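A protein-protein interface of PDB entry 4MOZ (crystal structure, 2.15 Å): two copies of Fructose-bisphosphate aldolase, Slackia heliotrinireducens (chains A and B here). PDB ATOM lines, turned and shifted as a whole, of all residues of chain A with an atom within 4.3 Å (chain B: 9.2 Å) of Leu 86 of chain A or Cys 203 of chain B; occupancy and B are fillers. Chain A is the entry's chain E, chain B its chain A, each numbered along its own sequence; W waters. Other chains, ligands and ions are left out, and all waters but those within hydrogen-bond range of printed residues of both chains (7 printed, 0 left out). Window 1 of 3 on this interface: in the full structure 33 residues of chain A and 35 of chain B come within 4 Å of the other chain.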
ATOM      1  N   CYS A  42       1.802 -31.933  -9.358  1.00  0.00           N
ATOM      2  CA  CYS A  42       1.727 -30.481  -9.542  1.00  0.00           C
ATOM      3  C   CYS A  42       2.478 -30.029 -10.783  1.00  0.00           C
ATOM      4  O   CYS A  42       3.013 -28.917 -10.823  1.00  0.00           O
ATOM      5  CB  CYS A  42       2.299 -29.764  -8.322  1.00  0.00           C
ATOM      6  SG  CYS A  42       1.445 -30.149  -6.785  1.00  0.00           S
ATOM      7  N   LYS A  45       0.844 -27.362 -14.944  1.00  0.00           N
ATOM      8  CA  LYS A  45       0.932 -25.991 -15.465  1.00  0.00           C
ATOM      9  C   LYS A  45       1.611 -25.939 -16.835  1.00  0.00           C
ATOM     10  O   LYS A  45       1.366 -25.026 -17.623  1.00  0.00           O
ATOM     11  CB  LYS A  45       1.649 -25.059 -14.489  1.00  0.00           C
ATOM     12  CG  LYS A  45       0.859 -24.742 -13.229  1.00  0.00           C
ATOM     13  CD  LYS A  45       1.676 -23.940 -12.220  1.00  0.00           C
ATOM     14  CE  LYS A  45       1.866 -22.491 -12.653  1.00  0.00           C
ATOM     15  NZ  LYS A  45       0.584 -21.754 -12.829  1.00  0.00           N
ATOM     16  N   VAL A  46       2.468 -26.915 -17.119  1.00  0.00           N
ATOM     17  CA  VAL A  46       3.032 -27.050 -18.458  1.00  0.00           C
ATOM     18  C   VAL A  46       2.121 -27.947 -19.296  1.00  0.00           C
ATOM     19  O   VAL A  46       1.662 -27.545 -20.371  1.00  0.00           O
ATOM     20  CB  VAL A  46       4.473 -27.606 -18.442  1.00  0.00           C
ATOM     21  CG1 VAL A  46       5.063 -27.586 -19.847  1.00  0.00           C
ATOM     22  CG2 VAL A  46       5.351 -26.806 -17.489  1.00  0.00           C
ATOM     23  N   PHE A  69       1.675 -25.556  -3.015  1.00  0.00           N
ATOM     24  CA  PHE A  69       2.635 -25.758  -1.935  1.00  0.00           C
ATOM     25  C   PHE A  69       1.955 -25.730  -0.575  1.00  0.00           C
ATOM     26  O   PHE A  69       2.365 -26.443   0.341  1.00  0.00           O
ATOM     27  CB  PHE A  69       3.756 -24.715  -2.002  1.00  0.00           C
ATOM     28  CG  PHE A  69       4.709 -24.924  -3.151  1.00  0.00           C
ATOM     29  CD1 PHE A  69       4.418 -24.420  -4.417  1.00  0.00           C
ATOM     30  CD2 PHE A  69       5.895 -25.631  -2.967  1.00  0.00           C
ATOM     31  CE1 PHE A  69       5.294 -24.613  -5.475  1.00  0.00           C
ATOM     32  CE2 PHE A  69       6.774 -25.827  -4.021  1.00  0.00           C
ATOM     33  CZ  PHE A  69       6.473 -25.317  -5.276  1.00  0.00           C
ATOM     34  N   GLN A  83       7.919 -29.372 -11.607  1.00  0.00           N
ATOM     35  CA  GLN A  83       9.103 -28.985 -12.369  1.00  0.00           C
ATOM     36  C   GLN A  83      10.167 -28.377 -11.456  1.00  0.00           C
ATOM     37  O   GLN A  83       9.847 -27.814 -10.406  1.00  0.00           O
ATOM     38  CB  GLN A  83       8.735 -28.008 -13.487  1.00  0.00           C
ATOM     39  CG  GLN A  83       8.000 -28.641 -14.668  1.00  0.00           C
ATOM     40  CD  GLN A  83       6.505 -28.814 -14.425  1.00  0.00           C
ATOM     41  OE1 GLN A  83       5.968 -28.379 -13.398  1.00  0.00           O
ATOM     42  NE2 GLN A  83       5.824 -29.448 -15.377  1.00  0.00           N
ATOM     43  N   ARG A  84      11.427 -28.509 -11.865  1.00  0.00           N
ATOM     44  CA  ARG A  84      12.569 -27.965 -11.127  1.00  0.00           C
ATOM     45  C   ARG A  84      12.375 -26.485 -10.809  1.00  0.00           C
ATOM     46  O   ARG A  84      12.584 -26.060  -9.672  1.00  0.00           O
ATOM     47  CB  ARG A  84      13.857 -28.159 -11.937  1.00  0.00           C
ATOM     48  CG  ARG A  84      15.151 -27.825 -11.206  1.00  0.00           C
ATOM     49  CD  ARG A  84      16.235 -27.390 -12.183  1.00  0.00           C
ATOM     50  NE  ARG A  84      15.804 -26.207 -12.927  1.00  0.00           N
ATOM     51  CZ  ARG A  84      16.022 -24.950 -12.549  1.00  0.00           C
ATOM     52  NH1 ARG A  84      16.699 -24.690 -11.437  1.00  0.00           N
ATOM     53  NH2 ARG A  84      15.567 -23.947 -13.290  1.00  0.00           N
ATOM     54  N   GLY A  85      11.967 -25.716 -11.819  1.00  0.00           N
ATOM     55  CA  GLY A  85      11.803 -24.273 -11.696  1.00  0.00           C
ATOM     56  C   GLY A  85      10.687 -23.862 -10.754  1.00  0.00           C
ATOM     57  O   GLY A  85      10.844 -22.909  -9.987  1.00  0.00           O
ATOM     58  N   LEU A  86       9.564 -24.579 -10.814  1.00  0.00           N
ATOM     59  CA  LEU A  86       8.435 -24.343  -9.915  1.00  0.00           C
ATOM     60  C   LEU A  86       8.854 -24.555  -8.458  1.00  0.00           C
ATOM     61  O   LEU A  86       8.601 -23.706  -7.596  1.00  0.00           O
ATOM     62  CB  LEU A  86       7.263 -25.269 -10.273  1.00  0.00           C
ATOM     63  CG  LEU A  86       5.974 -25.205  -9.441  1.00  0.00           C
ATOM     64  CD1 LEU A  86       5.326 -23.832  -9.528  1.00  0.00           C
ATOM     65  CD2 LEU A  86       4.998 -26.275  -9.902  1.00  0.00           C
ATOM     66  N   ILE A  87       9.506 -25.687  -8.208  1.00  0.00           N
ATOM     67  CA  ILE A  87      10.001 -26.036  -6.889  1.00  0.00           C
ATOM     68  C   ILE A  87      11.020 -24.991  -6.417  1.00  0.00           C
ATOM     69  O   ILE A  87      10.951 -24.527  -5.281  1.00  0.00           O
ATOM     70  CB  ILE A  87      10.570 -27.477  -6.881  1.00  0.00           C
ATOM     71  CG1 ILE A  87       9.419 -28.489  -6.984  1.00  0.00           C
ATOM     72  CG2 ILE A  87      11.406 -27.745  -5.635  1.00  0.00           C
ATOM     73  CD1 ILE A  87       9.849 -29.891  -7.350  1.00  0.00           C
ATOM     74  N   ALA A  88      11.923 -24.590  -7.308  1.00  0.00           N
ATOM     75  CA  ALA A  88      12.967 -23.611  -6.985  1.00  0.00           C
ATOM     76  C   ALA A  88      12.414 -22.289  -6.448  1.00  0.00           C
ATOM     77  O   ALA A  88      13.029 -21.666  -5.578  1.00  0.00           O
ATOM     78  CB  ALA A  88      13.858 -23.362  -8.194  1.00  0.00           C
ATOM     79  N   ARG A  89      11.254 -21.874  -6.953  1.00  0.00           N
ATOM     80  CA  ARG A  89      10.684 -20.576  -6.589  1.00  0.00           C
ATOM     81  C   ARG A  89       9.958 -20.545  -5.239  1.00  0.00           C
ATOM     82  O   ARG A  89       9.740 -19.465  -4.695  1.00  0.00           O
ATOM     83  CB  ARG A  89       9.752 -20.047  -7.690  1.00  0.00           C
ATOM     84  CG  ARG A  89      10.322 -20.073  -9.102  1.00  0.00           C
ATOM     85  CD  ARG A  89      11.477 -19.114  -9.305  1.00  0.00           C
ATOM     86  NE  ARG A  89      11.062 -17.716  -9.272  1.00  0.00           N
ATOM     87  CZ  ARG A  89      11.865 -16.695  -9.564  1.00  0.00           C
ATOM     88  NH1 ARG A  89      13.124 -16.916  -9.926  1.00  0.00           N
ATOM     89  NH2 ARG A  89      11.409 -15.452  -9.496  1.00  0.00           N
ATOM     90  N   TYR A  90       9.586 -21.707  -4.700  1.00  0.00           N
ATOM     91  CA  TYR A  90       8.799 -21.750  -3.463  1.00  0.00           C
ATOM     92  C   TYR A  90       9.397 -22.585  -2.328  1.00  0.00           C
ATOM     93  O   TYR A  90       9.031 -22.395  -1.168  1.00  0.00           O
ATOM     94  CB  TYR A  90       7.367 -22.227  -3.748  1.00  0.00           C
ATOM     95  CG  TYR A  90       6.557 -21.297  -4.629  1.00  0.00           C
ATOM     96  CD1 TYR A  90       6.585 -21.420  -6.015  1.00  0.00           C
ATOM     97  CD2 TYR A  90       5.755 -20.295  -4.075  1.00  0.00           C
ATOM     98  CE1 TYR A  90       5.844 -20.579  -6.828  1.00  0.00           C
ATOM     99  CE2 TYR A  90       5.008 -19.447  -4.883  1.00  0.00           C
ATOM    100  CZ  TYR A  90       5.061 -19.591  -6.260  1.00  0.00           C
ATOM    101  OH  TYR A  90       4.331 -18.757  -7.082  1.00  0.00           O
ATOM    102  N   PRO B  12      15.576 -17.576  -5.263  1.00  0.00           N
ATOM    103  CA  PRO B  12      15.057 -18.933  -5.470  1.00  0.00           C
ATOM    104  C   PRO B  12      16.109 -19.978  -5.112  1.00  0.00           C
ATOM    105  O   PRO B  12      17.306 -19.676  -5.114  1.00  0.00           O
ATOM    106  CB  PRO B  12      14.731 -18.967  -6.966  1.00  0.00           C
ATOM    107  CG  PRO B  12      15.642 -17.953  -7.575  1.00  0.00           C
ATOM    108  CD  PRO B  12      15.886 -16.894  -6.535  1.00  0.00           C
ATOM    109  N   ALA B  13      15.660 -21.194  -4.813  1.00  0.00           N
ATOM    110  CA  ALA B  13      16.530 -22.243  -4.282  1.00  0.00           C
ATOM    111  C   ALA B  13      17.574 -22.785  -5.270  1.00  0.00           C
ATOM    112  O   ALA B  13      18.485 -23.529  -4.874  1.00  0.00           O
ATOM    113  CB  ALA B  13      15.692 -23.374  -3.712  1.00  0.00           C
ATOM    114  N   ASP B  14      17.451 -22.415  -6.544  1.00  0.00           N
ATOM    115  CA  ASP B  14      18.443 -22.817  -7.551  1.00  0.00           C
ATOM    116  C   ASP B  14      19.582 -21.803  -7.711  1.00  0.00           C
ATOM    117  O   ASP B  14      20.517 -22.020  -8.487  1.00  0.00           O
ATOM    118  CB  ASP B  14      17.783 -23.147  -8.899  1.00  0.00           C
ATOM    119  CG  ASP B  14      17.050 -21.962  -9.517  1.00  0.00           C
ATOM    120  OD1 ASP B  14      16.729 -20.993  -8.796  1.00  0.00           O
ATOM    121  OD2 ASP B  14      16.782 -22.009 -10.737  1.00  0.00           O
ATOM    122  N   LEU B 156      12.203 -25.921 -25.129  1.00  0.00           N
ATOM    123  CA  LEU B 156      11.993 -26.260 -23.718  1.00  0.00           C
ATOM    124  C   LEU B 156      13.269 -26.814 -23.084  1.00  0.00           C
ATOM    125  O   LEU B 156      13.627 -26.437 -21.960  1.00  0.00           O
ATOM    126  CB  LEU B 156      10.835 -27.252 -23.545  1.00  0.00           C
ATOM    127  CG  LEU B 156       9.394 -26.747 -23.669  1.00  0.00           C
ATOM    128  CD1 LEU B 156       8.422 -27.923 -23.720  1.00  0.00           C
ATOM    129  CD2 LEU B 156       9.031 -25.813 -22.521  1.00  0.00           C
ATOM    130  N   ALA B 159      15.887 -23.922 -22.831  1.00  0.00           N
ATOM    131  CA  ALA B 159      15.494 -22.945 -21.811  1.00  0.00           C
ATOM    132  C   ALA B 159      15.658 -23.486 -20.383  1.00  0.00           C
ATOM    133  O   ALA B 159      16.200 -22.802 -19.506  1.00  0.00           O
ATOM    134  CB  ALA B 159      14.069 -22.470 -22.047  1.00  0.00           C
ATOM    135  N   GLY B 160      15.191 -24.711 -20.164  1.00  0.00           N
ATOM    136  CA  GLY B 160      15.266 -25.338 -18.855  1.00  0.00           C
ATOM    137  C   GLY B 160      16.684 -25.404 -18.325  1.00  0.00           C
ATOM    138  O   GLY B 160      16.936 -25.048 -17.177  1.00  0.00           O
ATOM    139  N   VAL B 163      18.147 -21.731 -17.595  1.00  0.00           N
ATOM    140  CA  VAL B 163      17.708 -21.154 -16.318  1.00  0.00           C
ATOM    141  C   VAL B 163      18.553 -21.688 -15.153  1.00  0.00           C
ATOM    142  O   VAL B 163      19.037 -20.911 -14.335  1.00  0.00           O
ATOM    143  CB  VAL B 163      16.202 -21.376 -16.052  1.00  0.00           C
ATOM    144  CG1 VAL B 163      15.828 -20.902 -14.656  1.00  0.00           C
ATOM    145  CG2 VAL B 163      15.363 -20.639 -17.085  1.00  0.00           C
ATOM    146  N   ALA B 164      18.740 -23.006 -15.101  1.00  0.00           N
ATOM    147  CA  ALA B 164      19.570 -23.644 -14.073  1.00  0.00           C
ATOM    148  C   ALA B 164      21.020 -23.135 -14.075  1.00  0.00           C
ATOM    149  O   ALA B 164      21.569 -22.804 -13.022  1.00  0.00           O
ATOM    150  CB  ALA B 164      19.538 -25.152 -14.233  1.00  0.00           C
ATOM    151  N   LEU B 175      12.325 -14.849 -19.822  1.00  0.00           N
ATOM    152  CA  LEU B 175      11.860 -15.685 -20.918  1.00  0.00           C
ATOM    153  C   LEU B 175      10.787 -14.965 -21.736  1.00  0.00           C
ATOM    154  O   LEU B 175       9.779 -14.523 -21.195  1.00  0.00           O
ATOM    155  CB  LEU B 175      11.344 -17.040 -20.406  1.00  0.00           C
ATOM    156  CG  LEU B 175      12.313 -17.999 -19.687  1.00  0.00           C
ATOM    157  CD1 LEU B 175      11.610 -19.306 -19.338  1.00  0.00           C
ATOM    158  CD2 LEU B 175      13.586 -18.281 -20.487  1.00  0.00           C
ATOM    159  N   ILE B 177       7.956 -15.684 -24.011  1.00  0.00           N
ATOM    160  CA  ILE B 177       7.159 -16.851 -24.381  1.00  0.00           C
ATOM    161  C   ILE B 177       6.017 -16.455 -25.312  1.00  0.00           C
ATOM    162  O   ILE B 177       5.026 -15.849 -24.890  1.00  0.00           O
ATOM    163  CB  ILE B 177       6.675 -17.661 -23.158  1.00  0.00           C
ATOM    164  CG1 ILE B 177       7.880 -18.086 -22.295  1.00  0.00           C
ATOM    165  CG2 ILE B 177       5.893 -18.882 -23.623  1.00  0.00           C
ATOM    166  CD1 ILE B 177       7.607 -19.162 -21.267  1.00  0.00           C
ATOM    167  N   ALA B 195      -2.008 -16.670 -20.432  1.00  0.00           N
ATOM    168  CA  ALA B 195      -1.931 -17.240 -19.087  1.00  0.00           C
ATOM    169  C   ALA B 195      -1.115 -18.533 -19.077  1.00  0.00           C
ATOM    170  O   ALA B 195      -0.268 -18.730 -18.207  1.00  0.00           O
ATOM    171  CB  ALA B 195      -3.324 -17.473 -18.518  1.00  0.00           C
ATOM    172  N   GLY B 196      -1.367 -19.400 -20.058  1.00  0.00           N
ATOM    173  CA  GLY B 196      -0.602 -20.631 -20.210  1.00  0.00           C
ATOM    174  C   GLY B 196       0.883 -20.341 -20.326  1.00  0.00           C
ATOM    175  O   GLY B 196       1.707 -20.980 -19.665  1.00  0.00           O
ATOM    176  N   ALA B 197       1.219 -19.358 -21.157  1.00  0.00           N
ATOM    177  CA  ALA B 197       2.605 -18.981 -21.397  1.00  0.00           C
ATOM    178  C   ALA B 197       3.290 -18.528 -20.113  1.00  0.00           C
ATOM    179  O   ALA B 197       4.417 -18.936 -19.827  1.00  0.00           O
ATOM    180  CB  ALA B 197       2.681 -17.895 -22.458  1.00  0.00           C
ATOM    181  N   ALA B 198       2.596 -17.694 -19.339  1.00  0.00           N
ATOM    182  CA  ALA B 198       3.138 -17.154 -18.094  1.00  0.00           C
ATOM    183  C   ALA B 198       3.421 -18.262 -17.075  1.00  0.00           C
ATOM    184  O   ALA B 198       4.462 -18.253 -16.408  1.00  0.00           O
ATOM    185  CB  ALA B 198       2.191 -16.113 -17.516  1.00  0.00           C
ATOM    186  N   GLY B 199       2.497 -19.212 -16.967  1.00  0.00           N
ATOM    187  CA  GLY B 199       2.660 -20.355 -16.071  1.00  0.00           C
ATOM    188  C   GLY B 199       3.846 -21.242 -16.407  1.00  0.00           C
ATOM    189  O   GLY B 199       4.509 -21.767 -15.508  1.00  0.00           O
ATOM    190  N   VAL B 200       4.119 -21.412 -17.700  1.00  0.00           N
ATOM    191  CA  VAL B 200       5.247 -22.237 -18.149  1.00  0.00           C
ATOM    192  C   VAL B 200       6.583 -21.644 -17.685  1.00  0.00           C
ATOM    193  O   VAL B 200       7.453 -22.367 -17.199  1.00  0.00           O
ATOM    194  CB  VAL B 200       5.228 -22.465 -19.684  1.00  0.00           C
ATOM    195  CG1 VAL B 200       6.530 -23.093 -20.170  1.00  0.00           C
ATOM    196  CG2 VAL B 200       4.055 -23.348 -20.084  1.00  0.00           C
ATOM    197  N   ALA B 201       6.728 -20.327 -17.812  1.00  0.00           N
ATOM    198  CA  ALA B 201       7.951 -19.631 -17.396  1.00  0.00           C
ATOM    199  C   ALA B 201       8.308 -19.866 -15.930  1.00  0.00           C
ATOM    200  O   ALA B 201       9.483 -20.024 -15.594  1.00  0.00           O
ATOM    201  CB  ALA B 201       7.834 -18.142 -17.672  1.00  0.00           C
ATOM    202  N   LEU B 202       7.294 -19.866 -15.067  1.00  0.00           N
ATOM    203  CA  LEU B 202       7.482 -20.173 -13.649  1.00  0.00           C
ATOM    204  C   LEU B 202       8.009 -21.593 -13.463  1.00  0.00           C
ATOM    205  O   LEU B 202       8.958 -21.812 -12.710  1.00  0.00           O
ATOM    206  CB  LEU B 202       6.174 -19.983 -12.870  1.00  0.00           C
ATOM    207  CG  LEU B 202       6.138 -20.437 -11.402  1.00  0.00           C
ATOM    208  CD1 LEU B 202       7.123 -19.662 -10.537  1.00  0.00           C
ATOM    209  CD2 LEU B 202       4.736 -20.310 -10.843  1.00  0.00           C
ATOM    210  N   CYS B 203       7.398 -22.549 -14.157  1.00  0.00           N
ATOM    211  CA  CYS B 203       7.809 -23.951 -14.050  1.00  0.00           C
ATOM    212  C   CYS B 203       9.247 -24.162 -14.511  1.00  0.00           C
ATOM    213  O   CYS B 203       9.949 -25.035 -13.992  1.00  0.00           O
ATOM    214  CB  CYS B 203       6.850 -24.851 -14.822  1.00  0.00           C
ATOM    215  SG  CYS B 203       5.187 -24.852 -14.111  1.00  0.00           S
ATOM    216  N   LEU B 204       9.680 -23.351 -15.475  1.00  0.00           N
ATOM    217  CA  LEU B 204      11.059 -23.388 -15.966  1.00  0.00           C
ATOM    218  C   LEU B 204      12.014 -22.652 -15.028  1.00  0.00           C
ATOM    219  O   LEU B 204      13.229 -22.844 -15.098  1.00  0.00           O
ATOM    220  CB  LEU B 204      11.159 -22.836 -17.397  1.00  0.00           C
ATOM    221  CG  LEU B 204      10.495 -23.687 -18.491  1.00  0.00           C
ATOM    222  CD1 LEU B 204      10.414 -22.923 -19.802  1.00  0.00           C
ATOM    223  CD2 LEU B 204      11.200 -25.026 -18.690  1.00  0.00           C
ATOM    224  N   GLY B 205      11.457 -21.819 -14.152  1.00  0.00           N
ATOM    225  CA  GLY B 205      12.237 -21.154 -13.113  1.00  0.00           C
ATOM    226  C   GLY B 205      12.649 -19.733 -13.431  1.00  0.00           C
ATOM    227  O   GLY B 205      13.534 -19.191 -12.774  1.00  0.00           O
ATOM    228  N   ALA B 206      12.012 -19.124 -14.429  1.00  0.00           N
ATOM    229  CA  ALA B 206      12.361 -17.760 -14.858  1.00  0.00           C
ATOM    230  C   ALA B 206      12.095 -16.716 -13.782  1.00  0.00           C
ATOM    231  O   ALA B 206      11.175 -16.863 -12.984  1.00  0.00           O
ATOM    232  CB  ALA B 206      11.614 -17.391 -16.129  1.00  0.00           C
ATOM    233  N   ASP B 207      12.907 -15.664 -13.765  1.00  0.00           N
ATOM    234  CA  ASP B 207      12.670 -14.530 -12.878  1.00  0.00           C
ATOM    235  C   ASP B 207      11.596 -13.609 -13.443  1.00  0.00           C
ATOM    236  O   ASP B 207      10.833 -13.012 -12.694  1.00  0.00           O
ATOM    237  CB  ASP B 207      13.961 -13.756 -12.653  1.00  0.00           C
ATOM    238  CG  ASP B 207      15.032 -14.609 -12.026  1.00  0.00           C
ATOM    239  OD1 ASP B 207      14.856 -14.993 -10.856  1.00  0.00           O
ATOM    240  OD2 ASP B 207      16.030 -14.925 -12.714  1.00  0.00           O
ATOM    241  N   VAL B 209       8.828 -13.153 -17.097  1.00  0.00           N
ATOM    242  CA  VAL B 209       8.291 -13.670 -18.352  1.00  0.00           C
ATOM    243  C   VAL B 209       7.700 -12.526 -19.175  1.00  0.00           C
ATOM    244  O   VAL B 209       6.913 -11.732 -18.666  1.00  0.00           O
ATOM    245  CB  VAL B 209       7.259 -14.811 -18.141  1.00  0.00           C
ATOM    246  CG1 VAL B 209       6.048 -14.346 -17.335  1.00  0.00           C
ATOM    247  CG2 VAL B 209       6.819 -15.399 -19.478  1.00  0.00           C
ATOM    248  N   ALA B 231      -1.179 -13.806 -12.334  1.00  0.00           N
ATOM    249  CA  ALA B 231      -1.464 -14.750 -11.261  1.00  0.00           C
ATOM    250  C   ALA B 231      -0.831 -16.115 -11.557  1.00  0.00           C
ATOM    251  O   ALA B 231      -0.120 -16.665 -10.713  1.00  0.00           O
ATOM    252  CB  ALA B 231      -2.966 -14.871 -11.039  1.00  0.00           C
ATOM    253  N   ALA B 232      -1.073 -16.630 -12.766  1.00  0.00           N
ATOM    254  CA  ALA B 232      -0.502 -17.900 -13.241  1.00  0.00           C
ATOM    255  C   ALA B 232       1.022 -17.959 -13.128  1.00  0.00           C
ATOM    256  O   ALA B 232       1.595 -19.019 -12.852  1.00  0.00           O
ATOM    257  CB  ALA B 232      -0.923 -18.158 -14.681  1.00  0.00           C
ATOM    258  N   ALA B 233       1.663 -16.814 -13.349  1.00  0.00           N
ATOM    259  CA  ALA B 233       3.117 -16.684 -13.274  1.00  0.00           C
ATOM    260  C   ALA B 233       3.661 -16.761 -11.844  1.00  0.00           C
ATOM    261  O   ALA B 233       4.855 -16.983 -11.651  1.00  0.00           O
ATOM    262  CB  ALA B 233       3.565 -15.393 -13.949  1.00  0.00           C
ATOM    263  N   GLY B 234       2.789 -16.571 -10.852  1.00  0.00           N
ATOM    264  CA  GLY B 234       3.172 -16.681  -9.443  1.00  0.00           C
ATOM    265  C   GLY B 234       4.320 -15.766  -9.062  1.00  0.00           C
ATOM    266  O   GLY B 234       4.236 -14.550  -9.231  1.00  0.00           O
ATOM    267  N   ARG B 235       5.402 -16.357  -8.563  1.00  0.00           N
ATOM    268  CA  ARG B 235       6.599 -15.602  -8.177  1.00  0.00           C
ATOM    269  C   ARG B 235       7.530 -15.243  -9.348  1.00  0.00           C
ATOM    270  O   ARG B 235       8.618 -14.707  -9.135  1.00  0.00           O
ATOM    271  CB  ARG B 235       7.374 -16.355  -7.094  1.00  0.00           C
ATOM    272  CG  ARG B 235       6.680 -16.364  -5.745  1.00  0.00           C
ATOM    273  CD  ARG B 235       7.501 -17.093  -4.691  1.00  0.00           C
ATOM    274  NE  ARG B 235       6.878 -16.967  -3.374  1.00  0.00           N
ATOM    275  CZ  ARG B 235       7.332 -17.519  -2.251  1.00  0.00           C
ATOM    276  NH1 ARG B 235       6.675 -17.325  -1.115  1.00  0.00           N
ATOM    277  NH2 ARG B 235       8.430 -18.265  -2.253  1.00  0.00           N
ATOM    278  N   THR B 236       7.111 -15.551 -10.573  1.00  0.00           N
ATOM    279  CA  THR B 236       7.794 -15.058 -11.769  1.00  0.00           C
ATOM    280  C   THR B 236       7.108 -13.764 -12.194  1.00  0.00           C
ATOM    281  O   THR B 236       5.911 -13.761 -12.469  1.00  0.00           O
ATOM    282  CB  THR B 236       7.754 -16.090 -12.924  1.00  0.00           C
ATOM    283  OG1 THR B 236       8.530 -17.241 -12.570  1.00  0.00           O
ATOM    284  CG2 THR B 236       8.301 -15.501 -14.227  1.00  0.00           C
HETATM  285  O   HOH W   1       3.171 -27.321 -13.182  1.00  0.00           O
HETATM  286  O   HOH W   2      14.329 -20.174 -10.252  1.00  0.00           O
HETATM  287  O   HOH W   3      12.123 -26.964 -14.950  1.00  0.00           O
HETATM  288  O   HOH W   4      14.397 -25.510 -15.490  1.00  0.00           O
HETATM  289  O   HOH W   5       0.658 -22.616 -17.663  1.00  0.00           O
HETATM  290  O   HOH W   6      11.257 -12.175 -10.029  1.00  0.00           O
HETATM  291  O   HOH W   7      10.779 -14.935  -6.562  1.00  0.00           O
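No position is printed for both chains.
O of Gly 199 of chain B lies within hydrogen-bond range of SG of Cys 203 of chain B (3.5 Å). The backbone carbonyl oxygen (O) of Ala 206 of chain B is in hydrogen-bond range of the side-chain hydroxyl (OG1) of Thr 236 of chain B (2.7 Å). The backbone NH of Ala 206 of chain B is in hydrogen-bond range of the backbone carbonyl oxygen of Ala 201 of chain B, 2.9 Å away.
Gly 199 of chain B touches Lys 45 of chain A. Cys 203 of chain B touches Lys 45 of chain A. CG2 of Val 46 of chain A touches CB of Cys 203 of chain B (3.6 Å). Arg 84 of chain A touches Val 163 of chain B (NH2 to CG1, 3.3 Å). Gly 85 of chain A touches Gly 205 of chain B. O of Ala 88 of chain A touches CA of Pro 12 of chain B, 3.4 Å away. CB of Ala 88 of chain A touches CG of Asp 14 of chain B (3.7 Å). CG of Arg 89 of chain A touches CD1 of Leu 202 of chain B, at 3.5 Å. Gly 205 of chain B touches Arg 89 of chain A. Gly 234 of chain B touches Tyr 90 of chain A (CA to OH, 3.4 Å).
Of chain B, only Leu 202 (3.4 Å) and Cys 203 (3.2 Å) come within 4 Å of Leu 86 of chain A. Of chain A, only Lys 45 (3.6 Å), Val 46 (3.6 Å), Gln 83 (3.3 Å), Gly 85 (3.0 Å) and Leu 86 (3.2 Å) come within 4 Å of Cys 203 of chain B. Of chain B, only Cys 203 comes within 4 Å of Gln 83 of chain A. Of the printed residues of chain B, Gly 85 of chain A touches Leu 202 (3.3 Å), Cys 203 (3.0 Å), Leu 204 (3.7 Å) and Gly 205 (3.5 Å). Printed residues of chain A within 4 Å of Gly 199 of chain B: Lys 45. Of the printed residues of chain A, Gly 205 of chain B touches Gly 85 and Arg 89. Printed residues of chain B within 4 Å of Arg 84 of chain A: Asp 14 (2.8 Å), Val 163 (3.3 Å), Ala 164 (3.8 Å) and Leu 204 (3.2 Å). Printed residues of chain B within 4 Å of Tyr 90 of chain A: Gly 234 (3.4 Å) and Arg 235 (3.0 Å).
Of the 12 printed residues of chain A, 9 touch a printed residue of chain B. Hydrophobic or aromatic side chains of chain A within 4 Å of the printed part of chain B: Val 46, Leu 86, Ala 88 and Tyr 90. Of the 30 printed residues of chain B, 15 touch a printed residue of chain A. Hydrophobic or aromatic side chains of chain B within 4 Å of the printed part of chain A: Pro 12, Ala 13, Val 163, Ala 164 and Leu 202. Among the printed residues, 26 pairs touch across the chains. Among the printed residues, Asp or Glu carboxylates within 4 Å of a Lys or Arg side-chain nitrogen of the other chain: Arg 84 of chain A with Asp 14 of chain B and Arg 89 of chain A with Asp 207 of chain B.
The backbone carbonyl oxygen (O) of Leu 202 of chain B sits at hydrogen-bond distance from the backbone NH (N) of Leu 86 of chain A. OH of Tyr 90 of chain A sits at hydrogen-bond distance from N of Arg 235 of chain B. OD2 of Asp 14 of chain B lies within salt-bridge range of NH1 of Arg 84 of chain A (2.8 Å). The backbone carbonyl oxygen (O) of Ala 232 of chain B lies within hydrogen-bond range of the side-chain amino group (NZ) of Lys 45 of chain A, 2.9 Å away. NH1 of Arg 89 of chain A is in salt-bridge range of OD1 of Asp 207 of chain B. O of Arg 235 of chain B sits at hydrogen-bond distance from NH2 of Arg 89 of chain A (2.9 Å). O of Cys 203 of chain B is in hydrogen-bond range of N of Leu 86 of chain A. O of Leu 202 of chain B sits close to O of Gly 85 of chain A (3.5 Å). The backbone carbonyl oxygen (O) of Cys 203 of chain B sits at hydrogen-bond distance from the backbone NH (N) of Gly 85 of chain A (3.0 Å). The side-chain sulfur (SG) of Cys 203 of chain B is in hydrogen-bond range of the side-chain amide oxygen (OE1) of Gln 83 of chain A, at 3.7 Å. O of Leu 204 of chain B is in hydrogen-bond range of NH2 of Arg 84 of chain A, 3.2 Å away. N of Ala 13 of chain B lies within hydrogen-bond range of O of Ala 88 of chain A (2.8 Å).
Water W1 lies within hydrogen-bond range of the backbone carbonyl oxygen of Cys 42 of chain A (2.9 Å), the backbone NH of Lys 45 of chain A (2.9 Å), the side-chain amide oxygen of Gln 83 of chain A (3.0 Å) and the side-chain sulfur of Cys 203 of chain B (3.3 Å). Water W4 lies within hydrogen-bond range of the backbone carbonyl oxygen of Leu 204 of chain B, the guanidinium group of Arg 84 of chain A and the backbone carbonyl oxygen of Gly 160 of chain B. Water W3 bridges O of Cys 203 of chain B (3.1 Å) and N of Gly 85 of chain A (3.4 Å).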
